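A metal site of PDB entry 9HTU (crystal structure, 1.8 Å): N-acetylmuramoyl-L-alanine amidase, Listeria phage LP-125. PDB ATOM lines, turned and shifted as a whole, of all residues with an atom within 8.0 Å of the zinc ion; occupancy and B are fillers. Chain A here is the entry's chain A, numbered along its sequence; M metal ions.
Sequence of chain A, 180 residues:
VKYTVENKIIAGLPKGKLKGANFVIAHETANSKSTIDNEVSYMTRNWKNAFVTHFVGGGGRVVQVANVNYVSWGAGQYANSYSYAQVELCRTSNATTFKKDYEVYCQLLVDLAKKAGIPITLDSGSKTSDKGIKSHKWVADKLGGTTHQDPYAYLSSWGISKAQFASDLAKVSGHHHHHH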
ATOM      1  N   ILE A  25      -9.517  10.099 -23.700  1.00  0.00           N
ATOM      2  CA  ILE A  25     -10.188  10.806 -22.579  1.00  0.00           C
ATOM      3  C   ILE A  25     -11.490  11.440 -23.065  1.00  0.00           C
ATOM      4  O   ILE A  25     -11.481  12.152 -24.135  1.00  0.00           O
ATOM      5  CB  ILE A  25      -9.287  11.850 -21.896  1.00  0.00           C
ATOM      6  CG1 ILE A  25      -7.922  11.285 -21.522  1.00  0.00           C
ATOM      7  CG2 ILE A  25      -9.994  12.399 -20.660  1.00  0.00           C
ATOM      8  CD1 ILE A  25      -7.993  10.063 -20.590  1.00  0.00           C
ATOM      9  N   ALA A  26     -12.551  11.189 -22.304  1.00  0.00           N
ATOM     10  CA  ALA A  26     -13.900  11.777 -22.449  1.00  0.00           C
ATOM     11  C   ALA A  26     -14.054  12.986 -21.515  1.00  0.00           C
ATOM     12  O   ALA A  26     -14.094  12.837 -20.243  1.00  0.00           O
ATOM     13  CB  ALA A  26     -14.960  10.736 -22.278  1.00  0.00           C
ATOM     14  N   HIS A  27     -14.130  14.179 -22.129  1.00  0.00           N
ATOM     15  CA  HIS A  27     -14.329  15.467 -21.425  1.00  0.00           C
ATOM     16  C   HIS A  27     -15.684  16.105 -21.762  1.00  0.00           C
ATOM     17  O   HIS A  27     -16.313  15.752 -22.800  1.00  0.00           O
ATOM     18  CB  HIS A  27     -13.253  16.515 -21.813  1.00  0.00           C
ATOM     19  CG  HIS A  27     -11.841  16.161 -21.524  1.00  0.00           C
ATOM     20  ND1 HIS A  27     -11.267  16.423 -20.294  1.00  0.00           N
ATOM     21  CD2 HIS A  27     -10.850  15.685 -22.294  1.00  0.00           C
ATOM     22  CE1 HIS A  27     -10.000  16.098 -20.326  1.00  0.00           C
ATOM     23  NE2 HIS A  27      -9.706  15.654 -21.522  1.00  0.00           N
ATOM     24  N   GLU A  28     -16.045  17.161 -21.024  1.00  0.00           N
ATOM     25  CA  GLU A  28     -17.008  18.177 -21.525  1.00  0.00           C
ATOM     26  C   GLU A  28     -16.521  19.546 -21.034  1.00  0.00           C
ATOM     27  O   GLU A  28     -15.662  19.599 -20.133  1.00  0.00           O
ATOM     28  CB  GLU A  28     -18.439  17.835 -21.174  1.00  0.00           C
ATOM     29  CG  GLU A  28     -18.773  17.884 -19.695  1.00  0.00           C
ATOM     30  CD  GLU A  28     -19.364  19.191 -19.184  1.00  0.00           C
ATOM     31  OE1 GLU A  28     -19.416  19.325 -17.939  1.00  0.00           O
ATOM     32  OE2 GLU A  28     -19.734  20.054 -19.988  1.00  0.00           O
ATOM     33  N   THR A  29     -16.999  20.608 -21.662  1.00  0.00           N
ATOM     34  CA  THR A  29     -16.434  21.971 -21.493  1.00  0.00           C
ATOM     35  C   THR A  29     -16.804  22.573 -20.137  1.00  0.00           C
ATOM     36  O   THR A  29     -16.077  23.482 -19.656  1.00  0.00           O
ATOM     37  CB  THR A  29     -16.892  22.933 -22.568  1.00  0.00           C
ATOM     38  OG1 THR A  29     -18.305  23.062 -22.380  1.00  0.00           O
ATOM     39  CG2 THR A  29     -16.496  22.483 -23.953  1.00  0.00           C
ATOM     40  N   ALA A  30     -17.870  22.084 -19.526  1.00  0.00           N
ATOM     41  CA  ALA A  30     -18.462  22.687 -18.321  1.00  0.00           C
ATOM     42  C   ALA A  30     -18.921  24.119 -18.612  1.00  0.00           C
ATOM     43  O   ALA A  30     -19.046  24.875 -17.674  1.00  0.00           O
ATOM     44  CB  ALA A  30     -17.487  22.659 -17.171  1.00  0.00           C
ATOM     45  N   VAL A  52      -6.817  19.963 -25.938  1.00  0.00           N
ATOM     46  CA  VAL A  52      -7.258  18.556 -26.168  1.00  0.00           C
ATOM     47  C   VAL A  52      -7.042  18.269 -27.647  1.00  0.00           C
ATOM     48  O   VAL A  52      -6.496  19.133 -28.318  1.00  0.00           O
ATOM     49  CB  VAL A  52      -8.721  18.343 -25.728  1.00  0.00           C
ATOM     50  CG1 VAL A  52      -8.860  18.480 -24.225  1.00  0.00           C
ATOM     51  CG2 VAL A  52      -9.692  19.208 -26.499  1.00  0.00           C
ATOM     52  N   GLY A  74      -4.547  17.978 -21.522  1.00  0.00           N
ATOM     53  CA  GLY A  74      -6.001  17.953 -21.277  1.00  0.00           C
ATOM     54  C   GLY A  74      -6.430  17.437 -19.931  1.00  0.00           C
ATOM     55  O   GLY A  74      -7.617  17.727 -19.568  1.00  0.00           O
ATOM     56  N   ALA A  75      -5.628  16.619 -19.260  1.00  0.00           N
ATOM     57  CA  ALA A  75      -6.141  15.894 -18.081  1.00  0.00           C
ATOM     58  C   ALA A  75      -5.049  15.660 -17.032  1.00  0.00           C
ATOM     59  O   ALA A  75      -5.128  14.613 -16.358  1.00  0.00           O
ATOM     60  CB  ALA A  75      -6.734  14.582 -18.504  1.00  0.00           C
ATOM     61  N   GLN A  86      -7.983  13.212 -26.800  1.00  0.00           N
ATOM     62  CA  GLN A  86      -8.793  13.791 -25.711  1.00  0.00           C
ATOM     63  C   GLN A  86      -9.937  14.531 -26.377  1.00  0.00           C
ATOM     64  O   GLN A  86      -9.676  15.505 -27.156  1.00  0.00           O
ATOM     65  CB  GLN A  86      -7.927  14.656 -24.796  1.00  0.00           C
ATOM     66  CG  GLN A  86      -6.791  13.896 -24.116  1.00  0.00           C
ATOM     67  CD  GLN A  86      -6.304  14.536 -22.844  1.00  0.00           C
ATOM     68  OE1 GLN A  86      -7.089  15.011 -22.021  1.00  0.00           O
ATOM     69  NE2 GLN A  86      -5.005  14.498 -22.629  1.00  0.00           N
ATOM     70  N   VAL A  87     -11.152  14.059 -26.123  1.00  0.00           N
ATOM     71  CA  VAL A  87     -12.372  14.493 -26.862  1.00  0.00           C
ATOM     72  C   VAL A  87     -13.321  15.238 -25.912  1.00  0.00           C
ATOM     73  O   VAL A  87     -13.714  14.675 -24.843  1.00  0.00           O
ATOM     74  CB  VAL A  87     -13.108  13.294 -27.489  1.00  0.00           C
ATOM     75  CG1 VAL A  87     -14.380  13.732 -28.204  1.00  0.00           C
ATOM     76  CG2 VAL A  87     -12.158  12.520 -28.381  1.00  0.00           C
ATOM     77  N   GLU A  88     -13.659  16.464 -26.287  1.00  0.00           N
ATOM     78  CA  GLU A  88     -14.407  17.382 -25.401  1.00  0.00           C
ATOM     79  C   GLU A  88     -15.775  17.746 -25.978  1.00  0.00           C
ATOM     80  O   GLU A  88     -15.839  18.470 -27.024  1.00  0.00           O
ATOM     81  CB  GLU A  88     -13.560  18.590 -25.059  1.00  0.00           C
ATOM     82  CG  GLU A  88     -14.195  19.406 -23.948  1.00  0.00           C
ATOM     83  CD  GLU A  88     -13.151  20.129 -23.126  1.00  0.00           C
ATOM     84  OE1 GLU A  88     -12.079  19.512 -22.901  1.00  0.00           O
ATOM     85  OE2 GLU A  88     -13.375  21.315 -22.770  1.00  0.00           O
ATOM     86  N   TYR A 105     -20.266  12.152 -30.448  1.00  0.00           N
ATOM     87  CA  TYR A 105     -19.313  11.986 -29.328  1.00  0.00           C
ATOM     88  C   TYR A 105     -18.976  10.496 -29.124  1.00  0.00           C
ATOM     89  O   TYR A 105     -17.776  10.114 -29.043  1.00  0.00           O
ATOM     90  CB  TYR A 105     -19.950  12.578 -28.084  1.00  0.00           C
ATOM     91  CG  TYR A 105     -19.110  12.629 -26.828  1.00  0.00           C
ATOM     92  CD1 TYR A 105     -17.915  13.342 -26.759  1.00  0.00           C
ATOM     93  CD2 TYR A 105     -19.617  12.108 -25.648  1.00  0.00           C
ATOM     94  CE1 TYR A 105     -17.221  13.495 -25.549  1.00  0.00           C
ATOM     95  CE2 TYR A 105     -18.955  12.251 -24.442  1.00  0.00           C
ATOM     96  CZ  TYR A 105     -17.766  12.948 -24.385  1.00  0.00           C
ATOM     97  OH  TYR A 105     -17.175  13.111 -23.150  1.00  0.00           O
ATOM     98  N   SER A 135     -13.173   8.644 -18.638  1.00  0.00           N
ATOM     99  CA  SER A 135     -13.645   9.976 -18.207  1.00  0.00           C
ATOM    100  C   SER A 135     -12.509  10.752 -17.546  1.00  0.00           C
ATOM    101  O   SER A 135     -11.564  10.158 -16.941  1.00  0.00           O
ATOM    102  CB  SER A 135     -14.830   9.815 -17.270  1.00  0.00           C
ATOM    103  OG  SER A 135     -14.390   9.266 -16.025  1.00  0.00           O
ATOM    104  N   HIS A 136     -12.590  12.067 -17.609  1.00  0.00           N
ATOM    105  CA  HIS A 136     -11.739  12.944 -16.772  1.00  0.00           C
ATOM    106  C   HIS A 136     -11.901  12.484 -15.325  1.00  0.00           C
ATOM    107  O   HIS A 136     -10.884  12.447 -14.583  1.00  0.00           O
ATOM    108  CB  HIS A 136     -12.099  14.426 -16.972  1.00  0.00           C
ATOM    109  CG  HIS A 136     -11.018  15.392 -16.617  1.00  0.00           C
ATOM    110  ND1 HIS A 136     -10.942  16.640 -17.175  1.00  0.00           N
ATOM    111  CD2 HIS A 136      -9.985  15.328 -15.719  1.00  0.00           C
ATOM    112  CE1 HIS A 136      -9.837  17.263 -16.752  1.00  0.00           C
ATOM    113  NE2 HIS A 136      -9.268  16.505 -15.805  1.00  0.00           N
ATOM    114  N   LYS A 137     -13.136  12.201 -14.892  1.00  0.00           N
ATOM    115  CA  LYS A 137     -13.403  11.738 -13.510  1.00  0.00           C
ATOM    116  C   LYS A 137     -12.484  10.567 -13.148  1.00  0.00           C
ATOM    117  O   LYS A 137     -11.891  10.523 -12.059  1.00  0.00           O
ATOM    118  CB  LYS A 137     -14.844  11.288 -13.292  1.00  0.00           C
ATOM    119  CG  LYS A 137     -15.140  10.891 -11.841  1.00  0.00           C
ATOM    120  CD  LYS A 137     -16.592  10.661 -11.492  1.00  0.00           C
ATOM    121  CE  LYS A 137     -16.738   9.913 -10.156  1.00  0.00           C
ATOM    122  NZ  LYS A 137     -15.867  10.466  -9.094  1.00  0.00           N
ATOM    123  N   THR A 146      -5.158  15.977 -11.319  1.00  0.00           N
ATOM    124  CA  THR A 146      -6.359  16.736 -11.711  1.00  0.00           C
ATOM    125  C   THR A 146      -7.462  16.295 -10.769  1.00  0.00           C
ATOM    126  O   THR A 146      -7.390  15.164 -10.258  1.00  0.00           O
ATOM    127  CB  THR A 146      -6.725  16.461 -13.179  1.00  0.00           C
ATOM    128  OG1 THR A 146      -7.807  17.291 -13.607  1.00  0.00           O
ATOM    129  CG2 THR A 146      -7.115  15.002 -13.399  1.00  0.00           C
ATOM    130  N   HIS A 148     -10.933  17.180 -11.854  1.00  0.00           N
ATOM    131  CA  HIS A 148     -12.192  17.330 -12.625  1.00  0.00           C
ATOM    132  C   HIS A 148     -12.984  16.021 -12.764  1.00  0.00           C
ATOM    133  O   HIS A 148     -12.409  14.900 -12.736  1.00  0.00           O
ATOM    134  CB  HIS A 148     -11.887  17.994 -13.966  1.00  0.00           C
ATOM    135  CG  HIS A 148     -11.498  19.390 -13.784  1.00  0.00           C
ATOM    136  ND1 HIS A 148     -12.443  20.369 -13.774  1.00  0.00           N
ATOM    137  CD2 HIS A 148     -10.312  19.966 -13.446  1.00  0.00           C
ATOM    138  CE1 HIS A 148     -11.857  21.515 -13.476  1.00  0.00           C
ATOM    139  NE2 HIS A 148     -10.550  21.287 -13.271  1.00  0.00           N
ATOM    140  N   GLN A 149     -14.299  16.168 -12.870  1.00  0.00           N
ATOM    141  CA  GLN A 149     -15.246  15.061 -12.722  1.00  0.00           C
ATOM    142  C   GLN A 149     -16.060  14.870 -13.995  1.00  0.00           C
ATOM    143  O   GLN A 149     -17.009  14.046 -13.988  1.00  0.00           O
ATOM    144  CB  GLN A 149     -16.119  15.374 -11.499  1.00  0.00           C
ATOM    145  CG  GLN A 149     -15.363  15.547 -10.172  1.00  0.00           C
ATOM    146  CD  GLN A 149     -14.907  14.222  -9.650  1.00  0.00           C
ATOM    147  OE1 GLN A 149     -15.709  13.370  -9.252  1.00  0.00           O
ATOM    148  NE2 GLN A 149     -13.612  14.020  -9.708  1.00  0.00           N
ATOM    149  N   ASP A 150     -15.725  15.559 -15.081  1.00  0.00           N
ATOM    150  CA  ASP A 150     -16.485  15.453 -16.357  1.00  0.00           C
ATOM    151  C   ASP A 150     -16.348  14.050 -16.939  1.00  0.00           C
ATOM    152  O   ASP A 150     -15.350  13.391 -16.740  1.00  0.00           O
ATOM    153  CB  ASP A 150     -16.068  16.559 -17.350  1.00  0.00           C
ATOM    154  CG  ASP A 150     -14.595  16.873 -17.469  1.00  0.00           C
ATOM    155  OD1 ASP A 150     -13.971  17.211 -16.442  1.00  0.00           O
ATOM    156  OD2 ASP A 150     -14.108  16.827 -18.620  1.00  0.00           O
ATOM    157  N   PRO A 151     -17.289  13.593 -17.791  1.00  0.00           N
ATOM    158  CA  PRO A 151     -18.424  14.409 -18.243  1.00  0.00           C
ATOM    159  C   PRO A 151     -19.760  14.082 -17.569  1.00  0.00           C
ATOM    160  O   PRO A 151     -20.820  14.405 -18.130  1.00  0.00           O
ATOM    161  CB  PRO A 151     -18.494  13.996 -19.714  1.00  0.00           C
ATOM    162  CG  PRO A 151     -18.208  12.490 -19.642  1.00  0.00           C
ATOM    163  CD  PRO A 151     -17.131  12.360 -18.567  1.00  0.00           C
HETATM  164 ZN    ZN M   1     -12.175  17.336 -18.611  1.00  0.00          ZN
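The zinc ion is bound by the side-chain carboxylate of Asp 150 (2.0 Å), a ring nitrogen (ND1) of His 136 (2.0 Å) and a ring nitrogen (ND1) of His 27 (2.1 Å). Slightly farther from the zinc ion lies the side-chain carboxylate (OD1) of Asp 150 (2.8 Å).
The side-chain carboxylate (OD2) of Asp 150 sits close to the backbone NH (N) of Glu 28. O of Asp 150 is in hydrogen-bond range of N of Lys 137 (3.1 Å). The backbone NH of His 136 sits at hydrogen-bond distance from the backbone carbonyl oxygen of Ala 26, at 3.1 Å. A ring nitrogen (NE2) of His 136 is in hydrogen-bond range of the side-chain hydroxyl of Thr 146 (2.8 Å). NE2 of His 27 is in hydrogen-bond range of OE1 of Gln 86 (2.7 Å). N of His 27 lies within hydrogen-bond range of O of Val 87. O of His 27 sits at hydrogen-bond distance from OH of Tyr 105, at 2.8 Å.
Within 4 Å of the zinc ion: His 27, His 136 and Asp 150. Along chain A the residues within 4 Å of the zinc ion span positions 27 to 150. The nearest printed residue that does not touch the zinc ion is Glu 28 (4.4 Å).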
